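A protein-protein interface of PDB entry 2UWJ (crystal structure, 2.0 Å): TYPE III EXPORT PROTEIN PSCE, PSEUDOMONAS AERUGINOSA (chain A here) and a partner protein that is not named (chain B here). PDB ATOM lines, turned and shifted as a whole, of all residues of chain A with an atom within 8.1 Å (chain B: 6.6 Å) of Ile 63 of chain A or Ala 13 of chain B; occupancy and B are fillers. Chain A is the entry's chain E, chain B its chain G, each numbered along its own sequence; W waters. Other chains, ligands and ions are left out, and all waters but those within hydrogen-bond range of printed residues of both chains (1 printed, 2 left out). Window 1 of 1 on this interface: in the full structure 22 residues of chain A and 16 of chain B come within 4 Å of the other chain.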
ATOM      1  N   THR A   6     -22.581  32.284  -6.417  1.00  0.00           N
ATOM      2  CA  THR A   6     -23.666  31.477  -5.877  1.00  0.00           C
ATOM      3  C   THR A   6     -24.115  31.922  -4.482  1.00  0.00           C
ATOM      4  O   THR A   6     -23.346  32.545  -3.730  1.00  0.00           O
ATOM      5  CB  THR A   6     -23.265  29.977  -5.817  1.00  0.00           C
ATOM      6  OG1 THR A   6     -22.230  29.809  -4.845  1.00  0.00           O
ATOM      7  CG2 THR A   6     -22.725  29.487  -7.189  1.00  0.00           C
ATOM      8  N   LEU A   8     -24.722  30.012  -1.894  1.00  0.00           N
ATOM      9  CA  LEU A   8     -23.897  29.322  -0.888  1.00  0.00           C
ATOM     10  C   LEU A   8     -22.631  30.150  -0.591  1.00  0.00           C
ATOM     11  O   LEU A   8     -22.269  30.367   0.559  1.00  0.00           O
ATOM     12  CB  LEU A   8     -23.506  27.917  -1.400  1.00  0.00           C
ATOM     13  CG  LEU A   8     -22.355  27.212  -0.645  1.00  0.00           C
ATOM     14  CD1 LEU A   8     -22.793  26.886   0.782  1.00  0.00           C
ATOM     15  CD2 LEU A   8     -22.008  25.912  -1.402  1.00  0.00           C
ATOM     16  N   GLU A   9     -21.942  30.621  -1.621  1.00  0.00           N
ATOM     17  CA  GLU A   9     -20.734  31.409  -1.371  1.00  0.00           C
ATOM     18  C   GLU A   9     -21.039  32.671  -0.548  1.00  0.00           C
ATOM     19  O   GLU A   9     -20.239  33.077   0.294  1.00  0.00           O
ATOM     20  CB  GLU A   9     -20.055  31.788  -2.697  1.00  0.00           C
ATOM     21  CG  GLU A   9     -19.421  30.582  -3.367  1.00  0.00           C
ATOM     22  CD  GLU A   9     -19.070  30.856  -4.816  1.00  0.00           C
ATOM     23  OE1 GLU A   9     -17.992  31.465  -5.067  1.00  0.00           O
ATOM     24  OE2 GLU A   9     -19.892  30.499  -5.685  1.00  0.00           O
ATOM     25  N   LEU A  12     -21.379  31.556   2.954  1.00  0.00           N
ATOM     26  CA  LEU A  12     -20.040  31.288   3.489  1.00  0.00           C
ATOM     27  C   LEU A  12     -19.126  32.521   3.645  1.00  0.00           C
ATOM     28  O   LEU A  12     -18.086  32.429   4.270  1.00  0.00           O
ATOM     29  CB  LEU A  12     -19.313  30.273   2.589  1.00  0.00           C
ATOM     30  CG  LEU A  12     -19.866  28.877   2.349  1.00  0.00           C
ATOM     31  CD1 LEU A  12     -19.037  28.222   1.223  1.00  0.00           C
ATOM     32  CD2 LEU A  12     -19.812  28.029   3.618  1.00  0.00           C
ATOM     33  N   LEU A  27     -21.296  16.938   6.267  1.00  0.00           N
ATOM     34  CA  LEU A  27     -20.708  16.186   5.153  1.00  0.00           C
ATOM     35  C   LEU A  27     -19.818  15.046   5.720  1.00  0.00           C
ATOM     36  O   LEU A  27     -19.871  13.909   5.267  1.00  0.00           O
ATOM     37  CB  LEU A  27     -19.849  17.132   4.284  1.00  0.00           C
ATOM     38  CG  LEU A  27     -20.618  18.203   3.471  1.00  0.00           C
ATOM     39  CD1 LEU A  27     -19.583  19.171   2.810  1.00  0.00           C
ATOM     40  CD2 LEU A  27     -21.549  17.508   2.412  1.00  0.00           C
ATOM     41  N   ALA A  56     -19.130  11.645  -3.911  1.00  0.00           N
ATOM     42  CA  ALA A  56     -19.845  12.944  -3.986  1.00  0.00           C
ATOM     43  C   ALA A  56     -19.593  13.735  -2.717  1.00  0.00           C
ATOM     44  O   ALA A  56     -19.354  14.923  -2.745  1.00  0.00           O
ATOM     45  CB  ALA A  56     -21.334  12.722  -4.136  1.00  0.00           C
ATOM     46  N   LEU A  57     -19.647  13.047  -1.581  1.00  0.00           N
ATOM     47  CA  LEU A  57     -19.410  13.687  -0.290  1.00  0.00           C
ATOM     48  C   LEU A  57     -17.960  14.149  -0.167  1.00  0.00           C
ATOM     49  O   LEU A  57     -17.701  15.277   0.301  1.00  0.00           O
ATOM     50  CB  LEU A  57     -19.772  12.702   0.839  1.00  0.00           C
ATOM     51  CG  LEU A  57     -21.268  12.498   1.064  1.00  0.00           C
ATOM     52  CD1 LEU A  57     -21.483  11.246   2.041  1.00  0.00           C
ATOM     53  CD2 LEU A  57     -21.859  13.777   1.673  1.00  0.00           C
ATOM     54  N   GLU A  58     -17.013  13.292  -0.567  1.00  0.00           N
ATOM     55  CA  GLU A  58     -15.586  13.684  -0.535  1.00  0.00           C
ATOM     56  C   GLU A  58     -15.409  14.889  -1.486  1.00  0.00           C
ATOM     57  O   GLU A  58     -14.627  15.774  -1.198  1.00  0.00           O
ATOM     58  CB  GLU A  58     -14.695  12.560  -1.052  1.00  0.00           C
ATOM     59  CG  GLU A  58     -14.480  11.472  -0.024  1.00  0.00           C
ATOM     60  CD  GLU A  58     -13.845  10.228  -0.612  1.00  0.00           C
ATOM     61  OE1 GLU A  58     -13.747  10.101  -1.863  1.00  0.00           O
ATOM     62  OE2 GLU A  58     -13.466   9.365   0.208  1.00  0.00           O
ATOM     63  N   GLY A  59     -16.113  14.886  -2.631  1.00  0.00           N
ATOM     64  CA  GLY A  59     -16.003  16.036  -3.532  1.00  0.00           C
ATOM     65  C   GLY A  59     -16.551  17.317  -2.866  1.00  0.00           C
ATOM     66  O   GLY A  59     -15.986  18.422  -2.997  1.00  0.00           O
ATOM     67  N   GLY A  60     -17.673  17.176  -2.165  1.00  0.00           N
ATOM     68  CA  GLY A  60     -18.243  18.328  -1.466  1.00  0.00           C
ATOM     69  C   GLY A  60     -17.284  18.912  -0.433  1.00  0.00           C
ATOM     70  O   GLY A  60     -17.177  20.133  -0.287  1.00  0.00           O
ATOM     71  N   LEU A  61     -16.609  18.037   0.323  1.00  0.00           N
ATOM     72  CA  LEU A  61     -15.651  18.477   1.351  1.00  0.00           C
ATOM     73  C   LEU A  61     -14.468  19.170   0.686  1.00  0.00           C
ATOM     74  O   LEU A  61     -13.951  20.186   1.178  1.00  0.00           O
ATOM     75  CB  LEU A  61     -15.167  17.264   2.180  1.00  0.00           C
ATOM     76  CG  LEU A  61     -16.275  16.793   3.154  1.00  0.00           C
ATOM     77  CD1 LEU A  61     -15.986  15.342   3.590  1.00  0.00           C
ATOM     78  CD2 LEU A  61     -16.299  17.713   4.395  1.00  0.00           C
ATOM     79  N   GLY A  62     -14.048  18.619  -0.447  1.00  0.00           N
ATOM     80  CA  GLY A  62     -12.944  19.218  -1.177  1.00  0.00           C
ATOM     81  C   GLY A  62     -13.362  20.596  -1.740  1.00  0.00           C
ATOM     82  O   GLY A  62     -12.616  21.559  -1.698  1.00  0.00           O
ATOM     83  N   ILE A  63     -14.561  20.721  -2.274  1.00  0.00           N
ATOM     84  CA  ILE A  63     -14.942  22.043  -2.774  1.00  0.00           C
ATOM     85  C   ILE A  63     -15.052  23.020  -1.567  1.00  0.00           C
ATOM     86  O   ILE A  63     -14.541  24.131  -1.625  1.00  0.00           O
ATOM     87  CB  ILE A  63     -16.258  21.949  -3.534  1.00  0.00           C
ATOM     88  CG1 ILE A  63     -16.009  21.128  -4.843  1.00  0.00           C
ATOM     89  CG2 ILE A  63     -16.865  23.420  -3.752  1.00  0.00           C
ATOM     90  CD1 ILE A  63     -17.257  20.601  -5.488  1.00  0.00           C
ATOM     91  N   LEU A  64     -15.691  22.595  -0.471  1.00  0.00           N
ATOM     92  CA  LEU A  64     -15.859  23.465   0.706  1.00  0.00           C
ATOM     93  C   LEU A  64     -14.510  23.989   1.216  1.00  0.00           C
ATOM     94  O   LEU A  64     -14.366  25.175   1.524  1.00  0.00           O
ATOM     95  CB  LEU A  64     -16.564  22.723   1.826  1.00  0.00           C
ATOM     96  CG  LEU A  64     -16.824  23.555   3.104  1.00  0.00           C
ATOM     97  CD1 LEU A  64     -17.683  24.842   2.788  1.00  0.00           C
ATOM     98  CD2 LEU A  64     -17.615  22.628   4.096  1.00  0.00           C
ATOM     99  N   SER A  65     -13.516  23.120   1.249  1.00  0.00           N
ATOM    100  CA  SER A  65     -12.184  23.532   1.672  1.00  0.00           C
ATOM    101  C   SER A  65     -11.639  24.604   0.778  1.00  0.00           C
ATOM    102  O   SER A  65     -11.067  25.572   1.263  1.00  0.00           O
ATOM    103  CB  SER A  65     -11.197  22.367   1.656  1.00  0.00           C
ATOM    104  OG  SER A  65     -11.515  21.506   2.717  1.00  0.00           O
ATOM    105  N   GLN A  66     -11.786  24.439  -0.524  1.00  0.00           N
ATOM    106  CA  GLN A  66     -11.299  25.462  -1.453  1.00  0.00           C
ATOM    107  C   GLN A  66     -12.114  26.774  -1.361  1.00  0.00           C
ATOM    108  O   GLN A  66     -11.564  27.881  -1.502  1.00  0.00           O
ATOM    109  CB  GLN A  66     -11.344  24.940  -2.889  1.00  0.00           C
ATOM    110  CG  GLN A  66     -10.179  25.469  -3.744  1.00  0.00           C
ATOM    111  CD  GLN A  66     -10.629  26.372  -4.886  1.00  0.00           C
ATOM    112  OE1 GLN A  66     -11.193  27.455  -4.674  1.00  0.00           O
ATOM    113  NE2 GLN A  66     -10.369  25.937  -6.111  1.00  0.00           N
ATOM    114  N   LEU A  67     -13.421  26.674  -1.127  1.00  0.00           N
ATOM    115  CA  LEU A  67     -14.234  27.895  -1.026  1.00  0.00           C
ATOM    116  C   LEU A  67     -13.924  28.727   0.252  1.00  0.00           C
ATOM    117  O   LEU A  67     -14.097  29.951   0.276  1.00  0.00           O
ATOM    118  CB  LEU A  67     -15.744  27.543  -1.034  1.00  0.00           C
ATOM    119  CG  LEU A  67     -16.298  26.887  -2.334  1.00  0.00           C
ATOM    120  CD1 LEU A  67     -17.835  26.678  -2.216  1.00  0.00           C
ATOM    121  CD2 LEU A  67     -16.014  27.777  -3.519  1.00  0.00           C
ATOM    122  N   THR A  68     -13.477  28.054   1.306  1.00  0.00           N
ATOM    123  CA  THR A  68     -13.242  28.709   2.575  1.00  0.00           C
ATOM    124  C   THR A  68     -11.803  28.874   2.984  1.00  0.00           C
ATOM    125  O   THR A  68     -11.543  29.344   4.089  1.00  0.00           O
ATOM    126  CB  THR A  68     -13.911  27.935   3.726  1.00  0.00           C
ATOM    127  OG1 THR A  68     -13.322  26.632   3.817  1.00  0.00           O
ATOM    128  CG2 THR A  68     -15.407  27.809   3.498  1.00  0.00           C
ATOM    129  N   GLU A  69     -10.862  28.492   2.133  1.00  0.00           N
ATOM    130  CA  GLU A  69      -9.473  28.607   2.533  1.00  0.00           C
ATOM    131  C   GLU A  69      -9.008  30.048   2.451  1.00  0.00           C
ATOM    132  O   GLU A  69      -9.345  30.762   1.488  1.00  0.00           O
ATOM    133  CB  GLU A  69      -8.592  27.724   1.671  1.00  0.00           C
ATOM    134  CG  GLU A  69      -8.263  28.306   0.334  1.00  0.00           C
ATOM    135  CD  GLU A  69      -7.452  27.336  -0.482  1.00  0.00           C
ATOM    136  OE1 GLU A  69      -7.047  27.703  -1.608  1.00  0.00           O
ATOM    137  OE2 GLU A  69      -7.226  26.199   0.009  1.00  0.00           O
ATOM    138  N   GLU B   8     -27.416  21.136  -0.816  1.00  0.00           N
ATOM    139  CA  GLU B   8     -26.140  21.776  -0.538  1.00  0.00           C
ATOM    140  C   GLU B   8     -24.992  21.191  -1.369  1.00  0.00           C
ATOM    141  O   GLU B   8     -24.080  21.918  -1.786  1.00  0.00           O
ATOM    142  CB  GLU B   8     -25.833  21.691   0.962  1.00  0.00           C
ATOM    143  CG  GLU B   8     -26.840  22.568   1.716  1.00  0.00           C
ATOM    144  CD  GLU B   8     -26.688  22.456   3.198  1.00  0.00           C
ATOM    145  OE1 GLU B   8     -26.120  23.392   3.808  1.00  0.00           O
ATOM    146  OE2 GLU B   8     -27.119  21.414   3.734  1.00  0.00           O
ATOM    147  N   LEU B   9     -25.025  19.882  -1.599  1.00  0.00           N
ATOM    148  CA  LEU B   9     -23.980  19.240  -2.407  1.00  0.00           C
ATOM    149  C   LEU B   9     -24.127  19.746  -3.838  1.00  0.00           C
ATOM    150  O   LEU B   9     -23.125  20.012  -4.500  1.00  0.00           O
ATOM    151  CB  LEU B   9     -24.112  17.724  -2.412  1.00  0.00           C
ATOM    152  CG  LEU B   9     -23.478  17.092  -1.167  1.00  0.00           C
ATOM    153  CD1 LEU B   9     -23.983  15.647  -1.053  1.00  0.00           C
ATOM    154  CD2 LEU B   9     -21.933  17.150  -1.291  1.00  0.00           C
ATOM    155  N   ALA B  10     -25.365  19.881  -4.317  1.00  0.00           N
ATOM    156  CA  ALA B  10     -25.538  20.409  -5.692  1.00  0.00           C
ATOM    157  C   ALA B  10     -24.973  21.841  -5.788  1.00  0.00           C
ATOM    158  O   ALA B  10     -24.399  22.227  -6.822  1.00  0.00           O
ATOM    159  CB  ALA B  10     -27.033  20.411  -6.104  1.00  0.00           C
ATOM    160  N   GLU B  11     -25.176  22.642  -4.742  1.00  0.00           N
ATOM    161  CA  GLU B  11     -24.646  24.022  -4.739  1.00  0.00           C
ATOM    162  C   GLU B  11     -23.145  24.049  -4.639  1.00  0.00           C
ATOM    163  O   GLU B  11     -22.455  24.902  -5.280  1.00  0.00           O
ATOM    164  CB  GLU B  11     -25.211  24.845  -3.571  1.00  0.00           C
ATOM    165  CG  GLU B  11     -26.702  25.083  -3.624  1.00  0.00           C
ATOM    166  CD  GLU B  11     -27.155  25.951  -2.431  1.00  0.00           C
ATOM    167  OE1 GLU B  11     -27.678  25.392  -1.444  1.00  0.00           O
ATOM    168  OE2 GLU B  11     -26.948  27.184  -2.469  1.00  0.00           O
ATOM    169  N   LEU B  12     -22.591  23.147  -3.816  1.00  0.00           N
ATOM    170  CA  LEU B  12     -21.139  23.059  -3.729  1.00  0.00           C
ATOM    171  C   LEU B  12     -20.596  22.693  -5.126  1.00  0.00           C
ATOM    172  O   LEU B  12     -19.621  23.263  -5.576  1.00  0.00           O
ATOM    173  CB  LEU B  12     -20.708  21.963  -2.737  1.00  0.00           C
ATOM    174  CG  LEU B  12     -20.750  22.402  -1.255  1.00  0.00           C
ATOM    175  CD1 LEU B  12     -20.727  21.118  -0.327  1.00  0.00           C
ATOM    176  CD2 LEU B  12     -19.569  23.367  -0.993  1.00  0.00           C
ATOM    177  N   ALA B  13     -21.225  21.731  -5.799  1.00  0.00           N
ATOM    178  CA  ALA B  13     -20.733  21.312  -7.113  1.00  0.00           C
ATOM    179  C   ALA B  13     -20.765  22.486  -8.131  1.00  0.00           C
ATOM    180  O   ALA B  13     -19.821  22.677  -8.919  1.00  0.00           O
ATOM    181  CB  ALA B  13     -21.579  20.136  -7.647  1.00  0.00           C
ATOM    182  N   LEU B  14     -21.862  23.248  -8.113  1.00  0.00           N
ATOM    183  CA  LEU B  14     -21.975  24.378  -9.050  1.00  0.00           C
ATOM    184  C   LEU B  14     -20.907  25.417  -8.737  1.00  0.00           C
ATOM    185  O   LEU B  14     -20.200  25.875  -9.633  1.00  0.00           O
ATOM    186  CB  LEU B  14     -23.372  24.987  -8.937  1.00  0.00           C
ATOM    187  CG  LEU B  14     -23.558  26.119  -9.972  1.00  0.00           C
ATOM    188  CD1 LEU B  14     -23.449  25.527 -11.401  1.00  0.00           C
ATOM    189  CD2 LEU B  14     -24.950  26.755  -9.737  1.00  0.00           C
ATOM    190  N   ALA B  15     -20.754  25.783  -7.453  1.00  0.00           N
ATOM    191  CA  ALA B  15     -19.736  26.775  -7.071  1.00  0.00           C
ATOM    192  C   ALA B  15     -18.374  26.243  -7.485  1.00  0.00           C
ATOM    193  O   ALA B  15     -17.557  26.959  -8.040  1.00  0.00           O
ATOM    194  CB  ALA B  15     -19.760  27.044  -5.533  1.00  0.00           C
ATOM    195  N   GLY B  16     -18.135  24.970  -7.211  1.00  0.00           N
ATOM    196  CA  GLY B  16     -16.870  24.346  -7.554  1.00  0.00           C
ATOM    197  C   GLY B  16     -16.569  24.228  -9.054  1.00  0.00           C
ATOM    198  O   GLY B  16     -15.397  24.266  -9.477  1.00  0.00           O
ATOM    199  N   SER B  17     -17.609  24.108  -9.854  1.00  0.00           N
ATOM    200  CA  SER B  17     -17.444  23.988 -11.311  1.00  0.00           C
ATOM    201  C   SER B  17     -16.838  25.275 -11.895  1.00  0.00           C
ATOM    202  O   SER B  17     -16.327  25.232 -13.003  1.00  0.00           O
ATOM    203  CB  SER B  17     -18.800  23.719 -12.008  1.00  0.00           C
ATOM    204  OG  SER B  17     -19.680  24.860 -11.952  1.00  0.00           O
ATOM    205  N   GLY B  18     -16.950  26.395 -11.185  1.00  0.00           N
ATOM    206  CA  GLY B  18     -16.405  27.656 -11.674  1.00  0.00           C
ATOM    207  C   GLY B  18     -15.062  27.958 -11.003  1.00  0.00           C
ATOM    208  O   GLY B  18     -14.420  28.990 -11.299  1.00  0.00           O
ATOM    209  N   CYS B  21     -12.780  22.908  -9.583  1.00  0.00           N
ATOM    210  CA  CYS B  21     -12.971  21.634  -8.864  1.00  0.00           C
ATOM    211  C   CYS B  21     -13.810  20.735  -9.754  1.00  0.00           C
ATOM    212  O   CYS B  21     -14.925  20.355  -9.401  1.00  0.00           O
ATOM    213  CB  CYS B  21     -13.679  21.857  -7.531  1.00  0.00           C
ATOM    214  SG  CYS B  21     -12.738  22.964  -6.441  1.00  0.00           S
ATOM    215  N   GLU B  24     -14.415  16.880  -8.572  1.00  0.00           N
ATOM    216  CA  GLU B  24     -15.391  16.919  -7.495  1.00  0.00           C
ATOM    217  C   GLU B  24     -16.806  17.193  -8.010  1.00  0.00           C
ATOM    218  O   GLU B  24     -17.756  16.493  -7.635  1.00  0.00           O
ATOM    219  CB  GLU B  24     -15.014  17.984  -6.445  1.00  0.00           C
ATOM    220  CG  GLU B  24     -13.641  17.709  -5.758  1.00  0.00           C
ATOM    221  CD  GLU B  24     -12.418  18.210  -6.558  1.00  0.00           C
ATOM    222  OE1 GLU B  24     -12.563  18.733  -7.675  1.00  0.00           O
ATOM    223  OE2 GLU B  24     -11.297  18.058  -6.054  1.00  0.00           O
ATOM    224  N   ALA B  25     -16.950  18.184  -8.892  1.00  0.00           N
ATOM    225  CA  ALA B  25     -18.262  18.547  -9.415  1.00  0.00           C
ATOM    226  C   ALA B  25     -18.860  17.373 -10.159  1.00  0.00           C
ATOM    227  O   ALA B  25     -20.050  17.072 -10.020  1.00  0.00           O
ATOM    228  CB  ALA B  25     -18.166  19.791 -10.395  1.00  0.00           C
ATOM    229  N   LEU B  26     -18.025  16.713 -10.951  1.00  0.00           N
ATOM    230  CA  LEU B  26     -18.475  15.561 -11.733  1.00  0.00           C
ATOM    231  C   LEU B  26     -18.992  14.412 -10.833  1.00  0.00           C
ATOM    232  O   LEU B  26     -20.023  13.798 -11.148  1.00  0.00           O
ATOM    233  CB  LEU B  26     -17.361  15.042 -12.632  1.00  0.00           C
ATOM    234  CG  LEU B  26     -17.751  13.832 -13.515  1.00  0.00           C
ATOM    235  CD1 LEU B  26     -18.886  14.263 -14.447  1.00  0.00           C
ATOM    236  CD2 LEU B  26     -16.526  13.299 -14.341  1.00  0.00           C
ATOM    237  N   ILE B  28     -20.266  14.690  -7.997  1.00  0.00           N
ATOM    238  CA  ILE B  28     -21.562  15.086  -7.459  1.00  0.00           C
ATOM    239  C   ILE B  28     -22.658  15.002  -8.505  1.00  0.00           C
ATOM    240  O   ILE B  28     -23.769  14.566  -8.217  1.00  0.00           O
ATOM    241  CB  ILE B  28     -21.511  16.507  -6.832  1.00  0.00           C
ATOM    242  CG1 ILE B  28     -20.627  16.438  -5.547  1.00  0.00           C
ATOM    243  CG2 ILE B  28     -22.977  16.988  -6.495  1.00  0.00           C
ATOM    244  CD1 ILE B  28     -20.125  17.808  -4.994  1.00  0.00           C
ATOM    245  N   ALA B  29     -22.346  15.394  -9.740  1.00  0.00           N
ATOM    246  CA  ALA B  29     -23.360  15.326 -10.793  1.00  0.00           C
ATOM    247  C   ALA B  29     -23.822  13.881 -11.026  1.00  0.00           C
ATOM    248  O   ALA B  29     -25.020  13.632 -11.225  1.00  0.00           O
ATOM    249  CB  ALA B  29     -22.817  15.904 -12.119  1.00  0.00           C
ATOM    250  N   LEU B  32     -26.125  12.952  -8.282  1.00  0.00           N
ATOM    251  CA  LEU B  32     -27.422  13.621  -8.447  1.00  0.00           C
ATOM    252  C   LEU B  32     -28.265  12.893  -9.513  1.00  0.00           C
ATOM    253  O   LEU B  32     -29.491  12.814  -9.404  1.00  0.00           O
ATOM    254  CB  LEU B  32     -27.256  15.097  -8.866  1.00  0.00           C
ATOM    255  CG  LEU B  32     -26.760  15.999  -7.732  1.00  0.00           C
ATOM    256  CD1 LEU B  32     -26.314  17.330  -8.368  1.00  0.00           C
ATOM    257  CD2 LEU B  32     -27.908  16.221  -6.680  1.00  0.00           C
ATOM    258  N   ILE B  44     -24.588  21.284 -13.795  1.00  0.00           N
ATOM    259  CA  ILE B  44     -23.222  21.151 -13.254  1.00  0.00           C
ATOM    260  C   ILE B  44     -22.238  20.614 -14.288  1.00  0.00           C
ATOM    261  O   ILE B  44     -21.129  21.143 -14.447  1.00  0.00           O
ATOM    262  CB  ILE B  44     -23.225  20.222 -11.976  1.00  0.00           C
ATOM    263  CG1 ILE B  44     -23.945  20.955 -10.799  1.00  0.00           C
ATOM    264  CG2 ILE B  44     -21.783  19.857 -11.580  1.00  0.00           C
ATOM    265  CD1 ILE B  44     -24.611  19.913  -9.716  1.00  0.00           C
ATOM    266  N   SER B  47     -21.605  23.447 -16.886  1.00  0.00           N
ATOM    267  CA  SER B  47     -20.809  24.514 -16.331  1.00  0.00           C
ATOM    268  C   SER B  47     -19.349  24.052 -16.181  1.00  0.00           C
ATOM    269  O   SER B  47     -18.398  24.797 -16.521  1.00  0.00           O
ATOM    270  CB  SER B  47     -21.360  24.953 -14.964  1.00  0.00           C
ATOM    271  OG  SER B  47     -20.501  25.919 -14.375  1.00  0.00           O
ATOM    272  N   SER B  48     -19.159  22.837 -15.680  1.00  0.00           N
ATOM    273  CA  SER B  48     -17.812  22.319 -15.469  1.00  0.00           C
ATOM    274  C   SER B  48     -17.077  22.203 -16.812  1.00  0.00           C
ATOM    275  O   SER B  48     -15.931  22.621 -16.926  1.00  0.00           O
ATOM    276  CB  SER B  48     -17.843  20.928 -14.839  1.00  0.00           C
ATOM    277  OG  SER B  48     -16.520  20.433 -14.801  1.00  0.00           O
HETATM  278  O   HOH W   1     -17.773  29.827  -7.608  1.00  0.00           O
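The side-chain hydroxyl (OG1) of Thr 6 of chain A is in hydrogen-bond range of the side-chain carboxylate (OE2) of Glu 9 of chain A, 2.6 Å away.
The backbone carbonyl oxygen (O) of Leu 64 of chain A sits at hydrogen-bond distance from the side-chain hydroxyl (OG1) of Thr 68 of chain A, at 2.9 Å.
O of Gly 16 of chain B is in hydrogen-bond range of N of Cys 21 of chain B (3.0 Å).
Thr 6 of chain A touches Ala 15 of chain B (OG1 to CB, 3.8 Å).
Leu 12 of chain B touches Leu 8 of chain A.
Glu 9 of chain A touches Ala 15 of chain B (OE2 to CB, 3.5 Å).
Leu 9 of chain B touches Leu 27 of chain A (CD2 to CD2, 3.7 Å).
Leu 9 of chain B touches Ala 56 of chain A (CD2 to O, 3.7 Å).
CD2 of Leu 57 of chain A touches CD1 of Leu 9 of chain B (3.9 Å).
Leu 12 of chain B touches Ile 63 of chain A (O to CG2, 3.3 Å).
Ile 63 of chain A touches Ala 13 of chain B (CD1 to CA, 3.9 Å).
Leu 64 of chain A touches Leu 12 of chain B.
CD1 of Leu 67 of chain A touches CD2 of Leu 12 of chain B, at 3.9 Å.
Ile 63 of chain A touches just these residues of chain B: Leu 12 (3.3 Å), Ala 13 (3.9 Å), Gly 16 (3.9 Å), Cys 21 (3.6 Å) and Glu 24 (3.6 Å).
Ala 13 of chain B touches just one residue of chain A: Ile 63.
Of the printed residues of chain B, Gly 59 of chain A touches Glu 24 (3.6 Å).
Printed residues of chain B within 4 Å of Thr 6 of chain A: Ala 15 (3.8 Å).
Printed residues of chain A within 4 Å of Leu 12 of chain B: Leu 8, Leu 27, Gly 60, Ile 63, Leu 64 and Leu 67.
Of the printed residues of chain A, Cys 21 of chain B touches Ile 63 and Gln 66.
Glu 8 of chain B touches none of the printed residues of chain A.
Leu 26 of chain B touches none of the printed residues of chain A.
The nearest residue of chain A that does not touch Ala 13 of chain B is Leu 8 of chain A (6.1 Å).
The nearest printed residue of chain A that does not touch Glu 24 of chain B is Gly 62 of chain A (4.9 Å).
Printed residues of chain B that touch a printed residue of chain A: Leu 9, Glu 11, Leu 12, Ala 13, Ala 15, Gly 16, Cys 21, Glu 24 and Ile 28.
Hydrophobic or aromatic side chains of chain B that line the printed part of chain A: Leu 9, Leu 12, Ala 15 and Ile 28.
Among the printed residues, 22 pairs touch across the chains.
Among the printed residues, no Asp or Glu carboxylate lies within 4 Å of a Lys or Arg side-chain nitrogen of the other chain.
Water W1 bridges O of Ala 15 of chain B (2.9 Å) and OE2 of Glu 9 of chain A (2.9 Å).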
